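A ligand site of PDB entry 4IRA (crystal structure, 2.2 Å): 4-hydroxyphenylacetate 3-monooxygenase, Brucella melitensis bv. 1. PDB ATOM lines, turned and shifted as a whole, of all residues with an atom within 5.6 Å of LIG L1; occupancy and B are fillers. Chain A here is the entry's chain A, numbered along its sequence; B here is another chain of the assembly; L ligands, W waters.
N4 of LIG L1 lies within hydrogen-bond range of OG of Ser 51 of chain B.
An oxygen (O6) of LIG L1 is in hydrogen-bond range of the side-chain carboxylate of Asp 54 of chain B (3.3 Å).
NE of Arg 166 lies within salt-bridge range of O13 of LIG L1 (3.3 Å).
O8 of LIG L1 is in hydrogen-bond range of NE2 of His 142 (3.5 Å).
The guanidinium group of Arg 20 is in salt-bridge range of an oxygen (O1) of LIG L1, 3.8 Å away.
O7 of LG2 L2 sits at hydrogen-bond distance from N of Gln 64 (3.1 Å).
The backbone NH (N) of Ala 48 lies within hydrogen-bond range of an oxygen (O8) of LG2 L2, 3.4 Å away.
A nitrogen (N8) of LG2 L2 sits at hydrogen-bond distance from the backbone NH (N) of Thr 47 (3.4 Å).
The side-chain hydroxyl (OH) of Tyr 19 sits at hydrogen-bond distance from the side-chain hydroxyl (OG) of Ser 51 of chain B (3.0 Å).
The side-chain carboxylate (OD2) of Asp 54 of chain B is in salt-bridge range of the guanidinium group (NH1) of Arg 20.
Met 23 touches LIG L1 (CB to O11, 3.8 Å).
Thr 47 touches LIG L1.
CB of Ala 48 touches O7 of LIG L1 (3.7 Å).
NE2 of Gln 64 touches O8 of LIG L1, at 3.6 Å.
Tyr 163 touches LIG L1 (CE2 to O10, 3.9 Å).
Hydrophobic or aromatic side chains that line LIG L1: Met 23, Ala 48 and Tyr 163.
Within 4 Å of LIG L1: Arg 20, Met 23, Thr 47, Ala 48, Gln 64, His 142, Tyr 163, Arg 166, Ser 51 of chain B and Asp 54 of chain B.
Along chain A the residues within 4 Å of LIG L1 span positions 20 to 166.
Water W7 lies within hydrogen-bond range of O7 of LIG L1 (2.7 Å) and OG1 of Thr 47 (3.1 Å).
Water W1 bridges an oxygen (O13) of LIG L1 (3.0 Å) and the guanidinium group of Arg 20 (3.4 Å).
Water W2 lies within hydrogen-bond range of O of Ser 51 of chain B, N7 of LIG L1, NE2 of His 142 and O of Val 52 of chain B.
Water W3 lies within hydrogen-bond range of the side-chain carboxylate of Asp 54 of chain B and an oxygen (O6) of LIG L1.
Water W8 lies within hydrogen-bond range of the backbone NH (N) of Arg 166 and an oxygen (O10) of LIG L1.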
ATOM      1  N   TYR A  19       0.767  18.974  17.877  1.00  0.00           N
ATOM      2  CA  TYR A  19      -0.310  19.012  16.834  1.00  0.00           C
ATOM      3  C   TYR A  19      -1.545  18.154  17.225  1.00  0.00           C
ATOM      4  O   TYR A  19      -2.689  18.645  17.123  1.00  0.00           O
ATOM      5  CB  TYR A  19       0.243  18.636  15.428  1.00  0.00           C
ATOM      6  CG  TYR A  19      -0.781  18.524  14.257  1.00  0.00           C
ATOM      7  CD1 TYR A  19      -1.341  19.683  13.648  1.00  0.00           C
ATOM      8  CD2 TYR A  19      -1.137  17.268  13.712  1.00  0.00           C
ATOM      9  CE1 TYR A  19      -2.272  19.576  12.570  1.00  0.00           C
ATOM     10  CE2 TYR A  19      -2.069  17.156  12.621  1.00  0.00           C
ATOM     11  CZ  TYR A  19      -2.629  18.319  12.049  1.00  0.00           C
ATOM     12  OH  TYR A  19      -3.536  18.221  10.990  1.00  0.00           O
ATOM     13  N   ARG A  20      -1.317  16.919  17.702  1.00  0.00           N
ATOM     14  CA  ARG A  20      -2.415  16.018  18.161  1.00  0.00           C
ATOM     15  C   ARG A  20      -3.221  16.501  19.397  1.00  0.00           C
ATOM     16  O   ARG A  20      -4.442  16.264  19.471  1.00  0.00           O
ATOM     17  CB  ARG A  20      -1.936  14.538  18.362  1.00  0.00           C
ATOM     18  CG  ARG A  20      -1.368  13.824  17.108  1.00  0.00           C
ATOM     19  CD  ARG A  20      -1.136  12.265  17.290  1.00  0.00           C
ATOM     20  NE  ARG A  20      -0.167  11.907  18.343  1.00  0.00           N
ATOM     21  CZ  ARG A  20       1.143  11.764  18.153  1.00  0.00           C
ATOM     22  NH1 ARG A  20       1.677  11.915  16.947  1.00  0.00           N
ATOM     23  NH2 ARG A  20       1.934  11.460  19.183  1.00  0.00           N
ATOM     24  N   MET A  23      -5.721  19.191  18.006  1.00  0.00           N
ATOM     25  CA  MET A  23      -6.784  18.498  17.244  1.00  0.00           C
ATOM     26  C   MET A  23      -7.827  17.763  18.123  1.00  0.00           C
ATOM     27  O   MET A  23      -8.920  17.442  17.634  1.00  0.00           O
ATOM     28  CB  MET A  23      -6.182  17.562  16.163  1.00  0.00           C
ATOM     29  CG  MET A  23      -5.799  18.247  14.807  1.00  0.00           C
ATOM     30  SD  MET A  23      -7.218  18.746  13.761  1.00  0.00           S
ATOM     31  CE  MET A  23      -7.796  17.181  13.164  1.00  0.00           C
ATOM     32  N   SER A  24      -7.508  17.504  19.409  1.00  0.00           N
ATOM     33  CA  SER A  24      -8.512  16.937  20.347  1.00  0.00           C
ATOM     34  C   SER A  24      -9.671  17.912  20.698  1.00  0.00           C
ATOM     35  O   SER A  24     -10.712  17.483  21.251  1.00  0.00           O
ATOM     36  CB  SER A  24      -7.863  16.313  21.622  1.00  0.00           C
ATOM     37  OG  SER A  24      -7.448  17.287  22.586  1.00  0.00           O
ATOM     38  N   THR A  47     -12.876   9.090  10.370  1.00  0.00           N
ATOM     39  CA  THR A  47     -13.323  10.519  10.457  1.00  0.00           C
ATOM     40  C   THR A  47     -12.773  11.533   9.397  1.00  0.00           C
ATOM     41  O   THR A  47     -13.401  12.586   9.179  1.00  0.00           O
ATOM     42  CB  THR A  47     -13.193  11.163  11.923  1.00  0.00           C
ATOM     43  OG1 THR A  47     -11.841  11.117  12.398  1.00  0.00           O
ATOM     44  CG2 THR A  47     -14.138  10.507  12.946  1.00  0.00           C
ATOM     45  N   ALA A  48     -11.643  11.236   8.743  1.00  0.00           N
ATOM     46  CA  ALA A  48     -11.038  12.171   7.741  1.00  0.00           C
ATOM     47  C   ALA A  48     -11.600  12.082   6.289  1.00  0.00           C
ATOM     48  O   ALA A  48     -10.981  11.472   5.405  1.00  0.00           O
ATOM     49  CB  ALA A  48      -9.502  12.032   7.732  1.00  0.00           C
ATOM     50  N   GLN A  64      -4.329   5.240   6.089  1.00  0.00           N
ATOM     51  CA  GLN A  64      -2.963   4.977   6.635  1.00  0.00           C
ATOM     52  C   GLN A  64      -2.089   3.958   5.836  1.00  0.00           C
ATOM     53  O   GLN A  64      -2.532   2.841   5.544  1.00  0.00           O
ATOM     54  CB  GLN A  64      -3.005   4.519   8.123  1.00  0.00           C
ATOM     55  CG  GLN A  64      -3.402   5.592   9.213  1.00  0.00           C
ATOM     56  CD  GLN A  64      -3.455   5.001  10.662  1.00  0.00           C
ATOM     57  OE1 GLN A  64      -2.721   4.065  10.991  1.00  0.00           O
ATOM     58  NE2 GLN A  64      -4.334   5.557  11.516  1.00  0.00           N
ATOM     59  N   HIS A 142      -0.060   9.053   4.405  1.00  0.00           N
ATOM     60  CA  HIS A 142      -1.398   8.571   3.928  1.00  0.00           C
ATOM     61  C   HIS A 142      -1.548   8.579   2.367  1.00  0.00           C
ATOM     62  O   HIS A 142      -0.869   9.367   1.688  1.00  0.00           O
ATOM     63  CB  HIS A 142      -2.541   9.460   4.507  1.00  0.00           C
ATOM     64  CG  HIS A 142      -2.826   9.295   5.988  1.00  0.00           C
ATOM     65  ND1 HIS A 142      -1.898   9.539   6.969  1.00  0.00           N
ATOM     66  CD2 HIS A 142      -3.989   8.988   6.632  1.00  0.00           C
ATOM     67  CE1 HIS A 142      -2.448   9.364   8.165  1.00  0.00           C
ATOM     68  NE2 HIS A 142      -3.725   9.034   7.989  1.00  0.00           N
ATOM     69  N   TYR A 163     -17.436  12.061  17.668  1.00  0.00           N
ATOM     70  CA  TYR A 163     -16.182  11.896  18.487  1.00  0.00           C
ATOM     71  C   TYR A 163     -15.498  13.262  18.835  1.00  0.00           C
ATOM     72  O   TYR A 163     -15.224  14.046  17.916  1.00  0.00           O
ATOM     73  CB  TYR A 163     -15.156  10.921  17.799  1.00  0.00           C
ATOM     74  CG  TYR A 163     -14.095  10.268  18.734  1.00  0.00           C
ATOM     75  CD1 TYR A 163     -14.424   9.179  19.551  1.00  0.00           C
ATOM     76  CD2 TYR A 163     -12.761  10.736  18.772  1.00  0.00           C
ATOM     77  CE1 TYR A 163     -13.464   8.566  20.395  1.00  0.00           C
ATOM     78  CE2 TYR A 163     -11.788  10.134  19.626  1.00  0.00           C
ATOM     79  CZ  TYR A 163     -12.158   9.045  20.437  1.00  0.00           C
ATOM     80  OH  TYR A 163     -11.239   8.438  21.288  1.00  0.00           O
ATOM     81  N   ARG A 166     -11.352  12.959  23.106  1.00  0.00           N
ATOM     82  CA  ARG A 166     -10.964  11.535  23.349  1.00  0.00           C
ATOM     83  C   ARG A 166     -12.078  10.585  23.910  1.00  0.00           C
ATOM     84  O   ARG A 166     -11.766   9.632  24.624  1.00  0.00           O
ATOM     85  CB  ARG A 166      -9.627  11.443  24.152  1.00  0.00           C
ATOM     86  CG  ARG A 166      -8.333  11.981  23.407  1.00  0.00           C
ATOM     87  CD  ARG A 166      -6.999  11.874  24.233  1.00  0.00           C
ATOM     88  NE  ARG A 166      -5.770  12.244  23.485  1.00  0.00           N
ATOM     89  CZ  ARG A 166      -5.089  13.391  23.616  1.00  0.00           C
ATOM     90  NH1 ARG A 166      -5.475  14.330  24.471  1.00  0.00           N
ATOM     91  NH2 ARG A 166      -3.991  13.615  22.889  1.00  0.00           N
ATOM     92  N   SER B  51      -8.016  17.012   8.150  1.00  0.00           N
ATOM     93  CA  SER B  51      -6.603  16.648   8.436  1.00  0.00           C
ATOM     94  C   SER B  51      -6.075  15.570   7.481  1.00  0.00           C
ATOM     95  O   SER B  51      -6.717  14.507   7.300  1.00  0.00           O
ATOM     96  CB  SER B  51      -6.478  16.170   9.899  1.00  0.00           C
ATOM     97  OG  SER B  51      -5.129  15.817  10.261  1.00  0.00           O
ATOM     98  N   VAL B  52      -4.896  15.835   6.887  1.00  0.00           N
ATOM     99  CA  VAL B  52      -4.205  14.925   5.922  1.00  0.00           C
ATOM    100  C   VAL B  52      -3.053  14.033   6.511  1.00  0.00           C
ATOM    101  O   VAL B  52      -3.009  12.825   6.225  1.00  0.00           O
ATOM    102  CB  VAL B  52      -3.688  15.717   4.648  1.00  0.00           C
ATOM    103  CG1 VAL B  52      -2.854  14.823   3.714  1.00  0.00           C
ATOM    104  CG2 VAL B  52      -4.861  16.354   3.867  1.00  0.00           C
ATOM    105  N   SER B  53      -2.124  14.633   7.277  1.00  0.00           N
ATOM    106  CA  SER B  53      -0.919  13.943   7.846  1.00  0.00           C
ATOM    107  C   SER B  53      -0.421  14.564   9.176  1.00  0.00           C
ATOM    108  O   SER B  53      -0.654  15.757   9.409  1.00  0.00           O
ATOM    109  CB  SER B  53       0.226  13.925   6.816  1.00  0.00           C
ATOM    110  OG  SER B  53       1.438  13.338   7.336  1.00  0.00           O
ATOM    111  N   ASP B  54       0.270  13.787  10.027  1.00  0.00           N
ATOM    112  CA  ASP B  54       0.939  14.329  11.251  1.00  0.00           C
ATOM    113  C   ASP B  54       2.495  14.382  11.237  1.00  0.00           C
ATOM    114  O   ASP B  54       3.124  14.702  12.279  1.00  0.00           O
ATOM    115  CB  ASP B  54       0.394  13.689  12.573  1.00  0.00           C
ATOM    116  CG  ASP B  54       0.874  12.216  12.787  1.00  0.00           C
ATOM    117  OD1 ASP B  54       1.384  11.580  11.835  1.00  0.00           O
ATOM    118  OD2 ASP B  54       0.705  11.692  13.921  1.00  0.00           O
HETATM  119  P1  LIG L   1      -3.300   8.299  19.017  1.00  0.00           P
HETATM  120  O1  LIG L   1      -2.053   8.891  19.659  1.00  0.00           O
HETATM  121  O2  LIG L   1      -3.856   7.150  19.805  1.00  0.00           O
HETATM  122  O3  LIG L   1      -2.838   7.859  17.522  1.00  0.00           O
HETATM  123  C1  LIG L   1      -3.325   6.711  16.825  1.00  0.00           C
HETATM  124  C2  LIG L   1      -2.806   6.638  15.380  1.00  0.00           C
HETATM  125  O4  LIG L   1      -3.524   7.488  14.479  1.00  0.00           O
HETATM  126  C3  LIG L   1      -1.344   7.046  15.266  1.00  0.00           C
HETATM  127  O5  LIG L   1      -0.702   6.167  14.375  1.00  0.00           O
HETATM  128  C4  LIG L   1      -1.380   8.425  14.663  1.00  0.00           C
HETATM  129  O6  LIG L   1      -0.259   8.568  13.833  1.00  0.00           O
HETATM  130  C5  LIG L   1      -2.713   8.513  13.901  1.00  0.00           C
HETATM  131  N1  LIG L   1      -3.381   9.860  14.039  1.00  0.00           N
HETATM  132  C6  LIG L   1      -4.011  10.299  15.185  1.00  0.00           C
HETATM  133  N2  LIG L   1      -4.511  11.553  14.966  1.00  0.00           N
HETATM  134  C7  LIG L   1      -4.223  11.938  13.702  1.00  0.00           C
HETATM  135  C8  LIG L   1      -4.513  13.117  12.981  1.00  0.00           C
HETATM  136  N3  LIG L   1      -5.294  14.063  13.528  1.00  0.00           N
HETATM  137  N4  LIG L   1      -4.086  13.245  11.658  1.00  0.00           N
HETATM  138  C9  LIG L   1      -3.387  12.188  11.068  1.00  0.00           C
HETATM  139  N5  LIG L   1      -3.111  11.025  11.789  1.00  0.00           N
HETATM  140  C10 LIG L   1      -3.512  10.880  13.095  1.00  0.00           C
HETATM  141  N6  LIG L   1      -8.029  11.463  12.818  1.00  0.00           N
HETATM  142  C11 LIG L   1      -7.566  11.733  11.527  1.00  0.00           C
HETATM  143  O7  LIG L   1      -7.865  12.820  10.992  1.00  0.00           O
HETATM  144  N7  LIG L   1      -6.774  10.797  10.851  1.00  0.00           N
HETATM  145  C12 LIG L   1      -6.446   9.584  11.451  1.00  0.00           C
HETATM  146  O8  LIG L   1      -5.742   8.753  10.816  1.00  0.00           O
HETATM  147  C13 LIG L   1      -6.920   9.321  12.771  1.00  0.00           C
HETATM  148  N8  LIG L   1      -6.617   8.131  13.401  1.00  0.00           N
HETATM  149  C14 LIG L   1      -7.063   7.858  14.692  1.00  0.00           C
HETATM  150  C15 LIG L   1      -6.707   6.634  15.289  1.00  0.00           C
HETATM  151  C16 LIG L   1      -7.142   6.322  16.590  1.00  0.00           C
HETATM  152  C17 LIG L   1      -6.740   4.995  17.201  1.00  0.00           C
HETATM  153  C18 LIG L   1      -7.933   7.234  17.293  1.00  0.00           C
HETATM  154  C19 LIG L   1      -8.398   6.899  18.685  1.00  0.00           C
HETATM  155  C20 LIG L   1      -8.289   8.459  16.697  1.00  0.00           C
HETATM  156  C21 LIG L   1      -7.850   8.792  15.385  1.00  0.00           C
HETATM  157  N9  LIG L   1      -8.181  10.021  14.769  1.00  0.00           N
HETATM  158  C22 LIG L   1      -7.715  10.271  13.457  1.00  0.00           C
HETATM  159  C23 LIG L   1      -9.083  11.038  15.485  1.00  0.00           C
HETATM  160  C24 LIG L   1      -8.495  12.325  16.127  1.00  0.00           C
HETATM  161  O9  LIG L   1      -7.998  13.206  15.133  1.00  0.00           O
HETATM  162  C25 LIG L   1      -7.566  11.990  17.335  1.00  0.00           C
HETATM  163  O10 LIG L   1      -8.375  11.627  18.446  1.00  0.00           O
HETATM  164  C26 LIG L   1      -6.501  13.031  17.783  1.00  0.00           C
HETATM  165  O11 LIG L   1      -6.044  13.844  16.738  1.00  0.00           O
HETATM  166  C27 LIG L   1      -5.194  12.322  18.104  1.00  0.00           C
HETATM  167  O12 LIG L   1      -5.075  11.934  19.448  1.00  0.00           O
HETATM  168  P2  LIG L   1      -5.152  10.390  19.923  1.00  0.00           P
HETATM  169  O13 LIG L   1      -4.374  10.318  21.220  1.00  0.00           O
HETATM  170  O14 LIG L   1      -6.611  10.047  20.124  1.00  0.00           O
HETATM  171  O15 LIG L   1      -4.438   9.454  18.789  1.00  0.00           O
HETATM  172  P1  LG2 L   2      -4.769  -5.033  12.842  1.00  0.00           P
HETATM  173  O1  LG2 L   2      -3.273  -4.903  12.716  1.00  0.00           O
HETATM  174  O2  LG2 L   2      -5.149  -4.768  14.282  1.00  0.00           O
HETATM  175  O3  LG2 L   2      -5.247  -6.505  12.391  1.00  0.00           O
HETATM  176  C1  LG2 L   2      -5.163  -7.009  11.066  1.00  0.00           C
HETATM  177  C2  LG2 L   2      -6.165  -8.140  10.781  1.00  0.00           C
HETATM  178  O4  LG2 L   2      -5.936  -9.332  11.519  1.00  0.00           O
HETATM  179  C3  LG2 L   2      -7.618  -7.788  11.092  1.00  0.00           C
HETATM  180  O5  LG2 L   2      -8.223  -7.013  10.079  1.00  0.00           O
HETATM  181  C4  LG2 L   2      -8.278  -9.153  11.212  1.00  0.00           C
HETATM  182  O6  LG2 L   2      -8.624  -9.601   9.924  1.00  0.00           O
HETATM  183  C5  LG2 L   2      -7.160 -10.043  11.763  1.00  0.00           C
HETATM  184  N1  LG2 L   2      -7.372 -10.298  13.227  1.00  0.00           N
HETATM  185  C6  LG2 L   2      -7.119  -9.409  14.249  1.00  0.00           C
HETATM  186  N2  LG2 L   2      -7.429  -9.999  15.431  1.00  0.00           N
HETATM  187  C7  LG2 L   2      -7.863 -11.258  15.190  1.00  0.00           C
HETATM  188  C8  LG2 L   2      -8.288 -12.284  16.044  1.00  0.00           C
HETATM  189  N3  LG2 L   2      -8.174 -12.159  17.373  1.00  0.00           N
HETATM  190  N4  LG2 L   2      -8.685 -13.505  15.517  1.00  0.00           N
HETATM  191  C9  LG2 L   2      -8.657 -13.694  14.148  1.00  0.00           C
HETATM  192  N5  LG2 L   2      -8.228 -12.676  13.297  1.00  0.00           N
HETATM  193  C10 LG2 L   2      -7.839 -11.467  13.807  1.00  0.00           C
HETATM  194  N6  LG2 L   2      -7.733   5.167  10.145  1.00  0.00           N
HETATM  195  C11 LG2 L   2      -7.473   5.763   8.900  1.00  0.00           C
HETATM  196  O7  LG2 L   2      -6.716   5.219   8.079  1.00  0.00           O
HETATM  197  N7  LG2 L   2      -8.071   6.978   8.572  1.00  0.00           N
HETATM  198  C12 LG2 L   2      -8.921   7.605   9.470  1.00  0.00           C
HETATM  199  O8  LG2 L   2      -9.437   8.685   9.123  1.00  0.00           O
HETATM  200  C13 LG2 L   2      -9.193   7.009  10.730  1.00  0.00           C
HETATM  201  N8  LG2 L   2     -10.058   7.622  11.643  1.00  0.00           N
HETATM  202  C14 LG2 L   2     -10.331   7.021  12.891  1.00  0.00           C
HETATM  203  C15 LG2 L   2     -11.205   7.642  13.807  1.00  0.00           C
HETATM  204  C16 LG2 L   2     -11.488   7.049  15.059  1.00  0.00           C
HETATM  205  C17 LG2 L   2     -12.434   7.713  16.046  1.00  0.00           C
HETATM  206  C18 LG2 L   2     -10.886   5.826  15.391  1.00  0.00           C
HETATM  207  C19 LG2 L   2     -11.176   5.170  16.728  1.00  0.00           C
HETATM  208  C20 LG2 L   2     -10.011   5.205  14.474  1.00  0.00           C
HETATM  209  C21 LG2 L   2      -9.714   5.781  13.221  1.00  0.00           C
HETATM  210  N9  LG2 L   2      -8.854   5.140  12.307  1.00  0.00           N
HETATM  211  C22 LG2 L   2      -8.582   5.769  11.069  1.00  0.00           C
HETATM  212  C23 LG2 L   2      -8.172   3.806  12.678  1.00  0.00           C
HETATM  213  C24 LG2 L   2      -8.671   2.490  12.029  1.00  0.00           C
HETATM  214  O9  LG2 L   2      -9.986   2.260  12.481  1.00  0.00           O
HETATM  215  C25 LG2 L   2      -7.759   1.254  12.317  1.00  0.00           C
HETATM  216  O10 LG2 L   2      -6.408   1.503  12.003  1.00  0.00           O
HETATM  217  C26 LG2 L   2      -8.087  -0.038  11.545  1.00  0.00           C
HETATM  218  O11 LG2 L   2      -9.405  -0.475  11.805  1.00  0.00           O
HETATM  219  C27 LG2 L   2      -7.106  -1.170  11.905  1.00  0.00           C
HETATM  220  O12 LG2 L   2      -7.199  -2.237  10.973  1.00  0.00           O
HETATM  221  P2  LG2 L   2      -7.055  -3.750  11.500  1.00  0.00           P
HETATM  222  O13 LG2 L   2      -7.942  -4.082  12.664  1.00  0.00           O
HETATM  223  O14 LG2 L   2      -7.508  -4.691  10.381  1.00  0.00           O
HETATM  224  O15 LG2 L   2      -5.456  -3.949  11.829  1.00  0.00           O
HETATM  225  O   HOH W   1      -1.613  11.468  21.392  1.00  0.00           O
HETATM  226  O   HOH W   2      -5.777  11.759   8.066  1.00  0.00           O
HETATM  227  O   HOH W   3       0.112   9.267  10.818  1.00  0.00           O
HETATM  228  O   HOH W   4      -7.782   8.564  22.240  1.00  0.00           O
HETATM  229  O   HOH W   5      -5.851   6.166  21.757  1.00  0.00           O
HETATM  230  O   HOH W   6       0.638   8.053  18.660  1.00  0.00           O
HETATM  231  O   HOH W   7     -10.357  13.680  11.664  1.00  0.00           O
HETATM  232  O   HOH W   8     -10.267  13.503  20.232  1.00  0.00           O
HETATM  233  O   HOH W   9      -3.809   9.099  23.721  1.00  0.00           O
